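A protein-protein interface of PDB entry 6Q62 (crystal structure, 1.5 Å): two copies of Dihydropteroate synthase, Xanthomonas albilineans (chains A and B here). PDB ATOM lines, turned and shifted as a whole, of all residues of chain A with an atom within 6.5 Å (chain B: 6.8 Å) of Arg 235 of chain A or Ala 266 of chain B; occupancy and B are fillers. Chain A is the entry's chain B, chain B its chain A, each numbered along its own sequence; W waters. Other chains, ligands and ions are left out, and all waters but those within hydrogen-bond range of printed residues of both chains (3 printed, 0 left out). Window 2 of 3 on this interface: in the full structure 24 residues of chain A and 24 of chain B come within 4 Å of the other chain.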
ATOM      1  N   LYS A 226     -31.441  19.786  -5.491  1.00  0.00           N
ATOM      2  CA  LYS A 226     -30.736  19.885  -4.232  1.00  0.00           C
ATOM      3  C   LYS A 226     -30.054  21.232  -4.043  1.00  0.00           C
ATOM      4  O   LYS A 226     -29.772  21.960  -5.021  1.00  0.00           O
ATOM      5  CB  LYS A 226     -29.789  18.712  -4.028  1.00  0.00           C
ATOM      6  CG  LYS A 226     -30.661  17.467  -3.745  1.00  0.00           C
ATOM      7  CD  LYS A 226     -29.918  16.380  -3.119  1.00  0.00           C
ATOM      8  CE  LYS A 226     -30.908  15.319  -2.797  1.00  0.00           C
ATOM      9  NZ  LYS A 226     -30.210  14.062  -2.653  1.00  0.00           N
ATOM     10  N   ARG A 227     -29.795  21.564  -2.770  1.00  0.00           N
ATOM     11  CA  ARG A 227     -29.171  22.841  -2.395  1.00  0.00           C
ATOM     12  C   ARG A 227     -27.850  23.067  -3.110  1.00  0.00           C
ATOM     13  O   ARG A 227     -27.611  24.191  -3.539  1.00  0.00           O
ATOM     14  CB  ARG A 227     -28.967  22.899  -0.867  1.00  0.00           C
ATOM     15  CG  ARG A 227     -28.391  24.236  -0.367  1.00  0.00           C
ATOM     16  CD  ARG A 227     -28.064  24.202   1.123  1.00  0.00           C
ATOM     17  NE  ARG A 227     -26.932  23.318   1.419  1.00  0.00           N
ATOM     18  CZ  ARG A 227     -25.655  23.697   1.465  1.00  0.00           C
ATOM     19  NH1 ARG A 227     -24.705  22.811   1.727  1.00  0.00           N
ATOM     20  NH2 ARG A 227     -25.324  24.972   1.285  1.00  0.00           N
ATOM     21  N   ILE A 229     -26.929  22.140  -6.076  1.00  0.00           N
ATOM     22  CA  ILE A 229     -27.224  22.573  -7.451  1.00  0.00           C
ATOM     23  C   ILE A 229     -27.597  24.050  -7.419  1.00  0.00           C
ATOM     24  O   ILE A 229     -27.131  24.838  -8.258  1.00  0.00           O
ATOM     25  CB  ILE A 229     -28.346  21.708  -8.113  1.00  0.00           C
ATOM     26  CG1 ILE A 229     -27.938  20.217  -8.174  1.00  0.00           C
ATOM     27  CG2 ILE A 229     -28.674  22.248  -9.500  1.00  0.00           C
ATOM     28  CD1 ILE A 229     -26.543  19.894  -8.858  1.00  0.00           C
ATOM     29  N   GLY A 230     -28.413  24.402  -6.425  1.00  0.00           N
ATOM     30  CA  GLY A 230     -28.832  25.775  -6.196  1.00  0.00           C
ATOM     31  C   GLY A 230     -27.658  26.701  -5.933  1.00  0.00           C
ATOM     32  O   GLY A 230     -27.602  27.794  -6.487  1.00  0.00           O
ATOM     33  N   GLU A 231     -26.682  26.250  -5.149  1.00  0.00           N
ATOM     34  CA  GLU A 231     -25.477  27.047  -4.838  1.00  0.00           C
ATOM     35  C   GLU A 231     -24.581  27.228  -6.075  1.00  0.00           C
ATOM     36  O   GLU A 231     -24.031  28.302  -6.277  1.00  0.00           O
ATOM     37  CB  GLU A 231     -24.675  26.417  -3.695  1.00  0.00           C
ATOM     38  CG  GLU A 231     -25.374  26.487  -2.339  1.00  0.00           C
ATOM     39  CD  GLU A 231     -25.414  27.820  -1.608  1.00  0.00           C
ATOM     40  OE1 GLU A 231     -26.297  27.989  -0.735  1.00  0.00           O
ATOM     41  OE2 GLU A 231     -24.572  28.698  -1.909  1.00  0.00           O
ATOM     42  N   LEU A 232     -24.437  26.188  -6.903  1.00  0.00           N
ATOM     43  CA  LEU A 232     -23.595  26.281  -8.093  1.00  0.00           C
ATOM     44  C   LEU A 232     -24.168  27.263  -9.128  1.00  0.00           C
ATOM     45  O   LEU A 232     -23.411  27.940  -9.798  1.00  0.00           O
ATOM     46  CB  LEU A 232     -23.451  24.885  -8.755  1.00  0.00           C
ATOM     47  CG  LEU A 232     -22.583  23.855  -8.028  1.00  0.00           C
ATOM     48  CD1 LEU A 232     -22.643  22.505  -8.754  1.00  0.00           C
ATOM     49  CD2 LEU A 232     -21.133  24.329  -7.911  1.00  0.00           C
ATOM     50  N   THR A 233     -25.498  27.304  -9.262  1.00  0.00           N
ATOM     51  CA  THR A 233     -26.212  28.071 -10.297  1.00  0.00           C
ATOM     52  C   THR A 233     -26.903  29.362  -9.839  1.00  0.00           C
ATOM     53  O   THR A 233     -27.434  30.115 -10.694  1.00  0.00           O
ATOM     54  CB  THR A 233     -27.273  27.167 -10.953  1.00  0.00           C
ATOM     55  OG1 THR A 233     -28.190  26.765  -9.959  1.00  0.00           O
ATOM     56  CG2 THR A 233     -26.672  25.958 -11.656  1.00  0.00           C
ATOM     57  N   GLY A 234     -26.944  29.575  -8.527  1.00  0.00           N
ATOM     58  CA  GLY A 234     -27.590  30.732  -7.913  1.00  0.00           C
ATOM     59  C   GLY A 234     -29.101  30.652  -7.990  1.00  0.00           C
ATOM     60  O   GLY A 234     -29.779  31.667  -8.160  1.00  0.00           O
ATOM     61  N   ARG A 235     -29.656  29.431  -7.884  1.00  0.00           N
ATOM     62  CA  ARG A 235     -31.110  29.223  -7.962  1.00  0.00           C
ATOM     63  C   ARG A 235     -31.628  28.839  -6.568  1.00  0.00           C
ATOM     64  O   ARG A 235     -31.344  27.749  -6.071  1.00  0.00           O
ATOM     65  CB  ARG A 235     -31.456  28.120  -8.993  1.00  0.00           C
ATOM     66  CG  ARG A 235     -30.912  28.409 -10.407  1.00  0.00           C
ATOM     67  CD  ARG A 235     -31.575  29.596 -11.114  1.00  0.00           C
ATOM     68  NE  ARG A 235     -30.937  29.774 -12.423  1.00  0.00           N
ATOM     69  CZ  ARG A 235     -30.945  30.908 -13.119  1.00  0.00           C
ATOM     70  NH1 ARG A 235     -31.598  31.970 -12.664  1.00  0.00           N
ATOM     71  NH2 ARG A 235     -30.324  30.978 -14.290  1.00  0.00           N
ATOM     72  N   GLU A 236     -32.352  29.751  -5.931  1.00  0.00           N
ATOM     73  CA  GLU A 236     -32.823  29.563  -4.566  1.00  0.00           C
ATOM     74  C   GLU A 236     -33.888  28.464  -4.341  1.00  0.00           C
ATOM     75  O   GLU A 236     -33.852  27.782  -3.317  1.00  0.00           O
ATOM     76  CB  GLU A 236     -33.364  30.889  -4.027  1.00  0.00           C
ATOM     77  CG  GLU A 236     -33.752  30.829  -2.555  1.00  0.00           C
ATOM     78  CD  GLU A 236     -34.731  31.892  -2.101  1.00  0.00           C
ATOM     79  OE1 GLU A 236     -34.959  32.862  -2.864  1.00  0.00           O
ATOM     80  OE2 GLU A 236     -35.259  31.754  -0.972  1.00  0.00           O
ATOM     81  N   LEU A 237     -34.882  28.403  -5.218  1.00  0.00           N
ATOM     82  CA  LEU A 237     -36.024  27.535  -5.002  1.00  0.00           C
ATOM     83  C   LEU A 237     -35.918  26.234  -5.799  1.00  0.00           C
ATOM     84  O   LEU A 237     -35.440  26.247  -6.923  1.00  0.00           O
ATOM     85  CB  LEU A 237     -37.332  28.286  -5.326  1.00  0.00           C
ATOM     86  CG  LEU A 237     -37.613  29.599  -4.533  1.00  0.00           C
ATOM     87  CD1 LEU A 237     -38.752  30.399  -5.176  1.00  0.00           C
ATOM     88  CD2 LEU A 237     -37.835  29.336  -3.030  1.00  0.00           C
ATOM     89  N   PRO A 238     -36.465  25.126  -5.264  1.00  0.00           N
ATOM     90  CA  PRO A 238     -36.329  23.834  -5.954  1.00  0.00           C
ATOM     91  C   PRO A 238     -36.696  23.817  -7.452  1.00  0.00           C
ATOM     92  O   PRO A 238     -35.895  23.297  -8.212  1.00  0.00           O
ATOM     93  CB  PRO A 238     -37.185  22.874  -5.117  1.00  0.00           C
ATOM     94  CG  PRO A 238     -37.128  23.473  -3.720  1.00  0.00           C
ATOM     95  CD  PRO A 238     -37.086  24.956  -3.917  1.00  0.00           C
ATOM     96  N   GLN A 240     -36.552  26.132  -9.528  1.00  0.00           N
ATOM     97  CA  GLN A 240     -35.632  26.959 -10.308  1.00  0.00           C
ATOM     98  C   GLN A 240     -34.361  26.174 -10.629  1.00  0.00           C
ATOM     99  O   GLN A 240     -33.553  26.628 -11.441  1.00  0.00           O
ATOM    100  CB  GLN A 240     -35.243  28.223  -9.521  1.00  0.00           C
ATOM    101  CG  GLN A 240     -36.392  29.181  -9.290  1.00  0.00           C
ATOM    102  CD  GLN A 240     -36.051  30.319  -8.356  1.00  0.00           C
ATOM    103  OE1 GLN A 240     -35.158  30.229  -7.516  1.00  0.00           O
ATOM    104  NE2 GLN A 240     -36.762  31.403  -8.487  1.00  0.00           N
ATOM    105  N   ARG A 241     -34.155  25.022  -9.961  1.00  0.00           N
ATOM    106  CA  ARG A 241     -32.941  24.210 -10.103  1.00  0.00           C
ATOM    107  C   ARG A 241     -33.069  23.086 -11.138  1.00  0.00           C
ATOM    108  O   ARG A 241     -32.203  22.204 -11.185  1.00  0.00           O
ATOM    109  CB  ARG A 241     -32.596  23.604  -8.732  1.00  0.00           C
ATOM    110  CG  ARG A 241     -32.291  24.668  -7.678  1.00  0.00           C
ATOM    111  CD  ARG A 241     -32.301  24.016  -6.311  1.00  0.00           C
ATOM    112  NE  ARG A 241     -32.078  25.006  -5.267  1.00  0.00           N
ATOM    113  CZ  ARG A 241     -32.206  24.740  -3.974  1.00  0.00           C
ATOM    114  NH1 ARG A 241     -32.527  23.513  -3.570  1.00  0.00           N
ATOM    115  NH2 ARG A 241     -31.961  25.683  -3.071  1.00  0.00           N
ATOM    116  N   VAL A 242     -34.124  23.102 -11.949  1.00  0.00           N
ATOM    117  CA  VAL A 242     -34.368  22.017 -12.919  1.00  0.00           C
ATOM    118  C   VAL A 242     -33.265  21.897 -13.970  1.00  0.00           C
ATOM    119  O   VAL A 242     -32.728  20.806 -14.163  1.00  0.00           O
ATOM    120  CB  VAL A 242     -35.772  22.140 -13.536  1.00  0.00           C
ATOM    121  CG1 VAL A 242     -36.000  21.062 -14.607  1.00  0.00           C
ATOM    122  CG2 VAL A 242     -36.829  22.042 -12.424  1.00  0.00           C
ATOM    123  N   ALA A 243     -32.885  23.021 -14.633  1.00  0.00           N
ATOM    124  CA  ALA A 243     -31.825  22.908 -15.640  1.00  0.00           C
ATOM    125  C   ALA A 243     -30.511  22.371 -15.092  1.00  0.00           C
ATOM    126  O   ALA A 243     -29.913  21.486 -15.697  1.00  0.00           O
ATOM    127  CB  ALA A 243     -31.617  24.243 -16.346  1.00  0.00           C
ATOM    128  N   VAL B  22     -21.976  31.534 -24.321  1.00  0.00           N
ATOM    129  CA  VAL B  22     -23.348  31.431 -24.795  1.00  0.00           C
ATOM    130  C   VAL B  22     -23.750  32.602 -25.639  1.00  0.00           C
ATOM    131  O   VAL B  22     -23.653  33.770 -25.208  1.00  0.00           O
ATOM    132  CB  VAL B  22     -24.315  31.196 -23.609  1.00  0.00           C
ATOM    133  CG1 VAL B  22     -25.784  31.175 -24.061  1.00  0.00           C
ATOM    134  CG2 VAL B  22     -23.967  29.889 -22.878  1.00  0.00           C
ATOM    135  N   LEU B  52     -32.161  38.132 -22.443  1.00  0.00           N
ATOM    136  CA  LEU B  52     -31.072  37.170 -22.620  1.00  0.00           C
ATOM    137  C   LEU B  52     -29.774  37.633 -21.952  1.00  0.00           C
ATOM    138  O   LEU B  52     -29.046  36.804 -21.385  1.00  0.00           O
ATOM    139  CB  LEU B  52     -30.868  36.820 -24.103  1.00  0.00           C
ATOM    140  CG  LEU B  52     -32.079  36.183 -24.815  1.00  0.00           C
ATOM    141  CD1 LEU B  52     -31.672  35.677 -26.184  1.00  0.00           C
ATOM    142  CD2 LEU B  52     -32.728  35.053 -23.979  1.00  0.00           C
ATOM    143  N   GLU B  55     -30.122  36.878 -18.389  1.00  0.00           N
ATOM    144  CA  GLU B  55     -30.000  35.440 -18.205  1.00  0.00           C
ATOM    145  C   GLU B  55     -28.558  34.947 -18.299  1.00  0.00           C
ATOM    146  O   GLU B  55     -28.311  33.772 -18.089  1.00  0.00           O
ATOM    147  CB  GLU B  55     -30.883  34.683 -19.209  1.00  0.00           C
ATOM    148  CG  GLU B  55     -32.358  34.862 -18.941  1.00  0.00           C
ATOM    149  CD  GLU B  55     -33.265  34.001 -19.785  1.00  0.00           C
ATOM    150  OE1 GLU B  55     -32.757  33.143 -20.539  1.00  0.00           O
ATOM    151  OE2 GLU B  55     -34.499  34.186 -19.683  1.00  0.00           O
ATOM    152  N   GLY B  56     -27.621  35.833 -18.640  1.00  0.00           N
ATOM    153  CA  GLY B  56     -26.216  35.467 -18.649  1.00  0.00           C
ATOM    154  C   GLY B  56     -25.593  35.178 -19.997  1.00  0.00           C
ATOM    155  O   GLY B  56     -24.509  34.595 -20.048  1.00  0.00           O
ATOM    156  N   ALA B  57     -26.237  35.596 -21.108  1.00  0.00           N
ATOM    157  CA  ALA B  57     -25.640  35.434 -22.443  1.00  0.00           C
ATOM    158  C   ALA B  57     -24.285  36.154 -22.455  1.00  0.00           C
ATOM    159  O   ALA B  57     -24.146  37.163 -21.768  1.00  0.00           O
ATOM    160  CB  ALA B  57     -26.542  36.084 -23.484  1.00  0.00           C
ATOM    161  N   VAL B 262     -27.938  29.652 -28.726  1.00  0.00           N
ATOM    162  CA  VAL B 262     -29.144  29.111 -28.074  1.00  0.00           C
ATOM    163  C   VAL B 262     -30.289  30.086 -27.900  1.00  0.00           C
ATOM    164  O   VAL B 262     -30.079  31.283 -27.750  1.00  0.00           O
ATOM    165  CB  VAL B 262     -28.770  28.492 -26.683  1.00  0.00           C
ATOM    166  CG1 VAL B 262     -27.500  27.637 -26.759  1.00  0.00           C
ATOM    167  CG2 VAL B 262     -28.594  29.572 -25.619  1.00  0.00           C
ATOM    168  N   HIS B 263     -31.520  29.534 -27.779  1.00  0.00           N
ATOM    169  CA  HIS B 263     -32.692  30.337 -27.415  1.00  0.00           C
ATOM    170  C   HIS B 263     -32.793  30.357 -25.871  1.00  0.00           C
ATOM    171  O   HIS B 263     -33.140  31.380 -25.289  1.00  0.00           O
ATOM    172  CB  HIS B 263     -33.989  29.670 -27.937  1.00  0.00           C
ATOM    173  CG  HIS B 263     -34.095  29.607 -29.423  1.00  0.00           C
ATOM    174  ND1 HIS B 263     -33.713  28.489 -30.117  1.00  0.00           N
ATOM    175  CD2 HIS B 263     -34.575  30.524 -30.298  1.00  0.00           C
ATOM    176  CE1 HIS B 263     -33.923  28.763 -31.401  1.00  0.00           C
ATOM    177  NE2 HIS B 263     -34.456  29.970 -31.555  1.00  0.00           N
ATOM    178  N   ASP B 264     -32.503  29.214 -25.222  1.00  0.00           N
ATOM    179  CA  ASP B 264     -32.711  29.013 -23.786  1.00  0.00           C
ATOM    180  C   ASP B 264     -31.457  29.315 -22.998  1.00  0.00           C
ATOM    181  O   ASP B 264     -30.696  28.421 -22.585  1.00  0.00           O
ATOM    182  CB  ASP B 264     -33.220  27.598 -23.555  1.00  0.00           C
ATOM    183  CG  ASP B 264     -34.480  27.394 -24.390  1.00  0.00           C
ATOM    184  OD1 ASP B 264     -35.530  27.948 -24.018  1.00  0.00           O
ATOM    185  OD2 ASP B 264     -34.390  26.747 -25.454  1.00  0.00           O
ATOM    186  N   VAL B 265     -31.201  30.620 -22.895  1.00  0.00           N
ATOM    187  CA  VAL B 265     -29.951  31.102 -22.303  1.00  0.00           C
ATOM    188  C   VAL B 265     -29.792  30.683 -20.846  1.00  0.00           C
ATOM    189  O   VAL B 265     -28.770  30.061 -20.532  1.00  0.00           O
ATOM    190  CB  VAL B 265     -29.769  32.608 -22.509  1.00  0.00           C
ATOM    191  CG1 VAL B 265     -28.546  33.125 -21.738  1.00  0.00           C
ATOM    192  CG2 VAL B 265     -29.629  32.926 -24.006  1.00  0.00           C
ATOM    193  N   ALA B 266     -30.723  31.037 -19.959  1.00  0.00           N
ATOM    194  CA  ALA B 266     -30.568  30.712 -18.524  1.00  0.00           C
ATOM    195  C   ALA B 266     -30.347  29.227 -18.289  1.00  0.00           C
ATOM    196  O   ALA B 266     -29.455  28.854 -17.524  1.00  0.00           O
ATOM    197  CB  ALA B 266     -31.800  31.187 -17.740  1.00  0.00           C
ATOM    198  N   ALA B 267     -31.119  28.366 -18.990  1.00  0.00           N
ATOM    199  CA  ALA B 267     -30.962  26.922 -18.818  1.00  0.00           C
ATOM    200  C   ALA B 267     -29.613  26.423 -19.283  1.00  0.00           C
ATOM    201  O   ALA B 267     -28.993  25.596 -18.594  1.00  0.00           O
ATOM    202  CB  ALA B 267     -32.083  26.181 -19.543  1.00  0.00           C
ATOM    203  N   THR B 268     -29.119  26.940 -20.437  1.00  0.00           N
ATOM    204  CA  THR B 268     -27.824  26.536 -20.953  1.00  0.00           C
ATOM    205  C   THR B 268     -26.701  27.014 -20.017  1.00  0.00           C
ATOM    206  O   THR B 268     -25.778  26.254 -19.726  1.00  0.00           O
ATOM    207  CB  THR B 268     -27.643  27.049 -22.414  1.00  0.00           C
ATOM    208  OG1 THR B 268     -28.738  26.581 -23.239  1.00  0.00           O
ATOM    209  CG2 THR B 268     -26.315  26.587 -23.024  1.00  0.00           C
ATOM    210  N   VAL B 269     -26.808  28.254 -19.515  1.00  0.00           N
ATOM    211  CA  VAL B 269     -25.809  28.774 -18.579  1.00  0.00           C
ATOM    212  C   VAL B 269     -25.746  27.885 -17.337  1.00  0.00           C
ATOM    213  O   VAL B 269     -24.667  27.505 -16.917  1.00  0.00           O
ATOM    214  CB  VAL B 269     -26.076  30.250 -18.233  1.00  0.00           C
ATOM    215  CG1 VAL B 269     -25.213  30.702 -17.043  1.00  0.00           C
ATOM    216  CG2 VAL B 269     -25.813  31.117 -19.462  1.00  0.00           C
ATOM    217  N   ASP B 270     -26.896  27.518 -16.796  1.00  0.00           N
ATOM    218  CA  ASP B 270     -26.938  26.624 -15.608  1.00  0.00           C
ATOM    219  C   ASP B 270     -26.269  25.288 -15.872  1.00  0.00           C
ATOM    220  O   ASP B 270     -25.445  24.823 -15.064  1.00  0.00           O
ATOM    221  CB  ASP B 270     -28.396  26.432 -15.173  1.00  0.00           C
ATOM    222  CG  ASP B 270     -28.970  27.631 -14.448  1.00  0.00           C
ATOM    223  OD1 ASP B 270     -28.330  28.711 -14.470  1.00  0.00           O
ATOM    224  OD2 ASP B 270     -30.062  27.512 -13.888  1.00  0.00           O
ATOM    225  N   ALA B 271     -26.566  24.674 -17.033  1.00  0.00           N
ATOM    226  CA  ALA B 271     -25.958  23.389 -17.374  1.00  0.00           C
ATOM    227  C   ALA B 271     -24.457  23.497 -17.498  1.00  0.00           C
ATOM    228  O   ALA B 271     -23.748  22.628 -17.009  1.00  0.00           O
ATOM    229  CB  ALA B 271     -26.530  22.849 -18.683  1.00  0.00           C
HETATM  230  O   HOH W   1     -29.089  32.961 -15.737  1.00  0.00           O
HETATM  231  O   HOH W   2     -26.413  30.138 -13.336  1.00  0.00           O
HETATM  232  O   HOH W   3     -31.452  25.376 -12.944  1.00  0.00           O
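The side-chain carboxylate (OD2) of Asp 270 of chain B is in salt-bridge range of the guanidinium group (NE) of Arg 235 of chain A (2.8 Å).
The side-chain hydroxyl (OG1) of Thr 233 of chain A lies within hydrogen-bond range of the backbone carbonyl oxygen (O) of Ile 229 of chain A (2.8 Å).
O of Arg 235 of chain A lies within hydrogen-bond range of NE of Arg 241 of chain A, 3.0 Å away.
The side-chain carboxylate of Glu 55 of chain B is in hydrogen-bond range of the backbone NH of Ala 266 of chain B.
The backbone NH (N) of Arg 235 of chain A sits at hydrogen-bond distance from the backbone carbonyl oxygen (O) of Gly 230 of chain A (3.0 Å).
Thr 233 of chain A touches Asp 270 of chain B (CG2 to O, 3.8 Å).
Ala 266 of chain B touches Arg 235 of chain A (CB to NH2, 3.8 Å).
CA of Ala 267 of chain B touches CB of Ala 243 of chain A, at 3.7 Å.
Arg 235 of chain A touches just these residues of chain B: Ala 266 and Asp 270.
Of chain A, only Arg 235 comes within 4 Å of Ala 266 of chain B.
Printed residues of chain A within 4 Å of Asp 270 of chain B: Thr 233 (3.8 Å) and Arg 235 (2.8 Å).
Printed residues of chain B within 4 Å of Thr 233 of chain A: Asp 270 (3.8 Å).
Of the printed residues of chain A, Ala 267 of chain B touches Ala 243.
Val 269 of chain B touches none of the printed residues of chain A.
The nearest printed residue of chain B that does not touch Thr 233 of chain A is Ala 271 of chain B (5.5 Å).
Hydrophobic or aromatic side chains of chain A that line the printed part of chain B: Ala 243.
No position is printed for both chains.
Water W1 bridges O of Glu 55 of chain B (2.6 Å) and NH2 of Arg 235 of chain A (2.7 Å).
Water W2 bridges the side-chain carboxylate (OD1) of Asp 270 of chain B (2.6 Å) and the backbone carbonyl oxygen (O) of Thr 233 of chain A (2.8 Å).
Water W3 lies within hydrogen-bond range of OD2 of Asp 270 of chain B (2.7 Å), O of Gln 240 of chain A (2.9 Å) and N of Ala 243 of chain A (3.2 Å).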
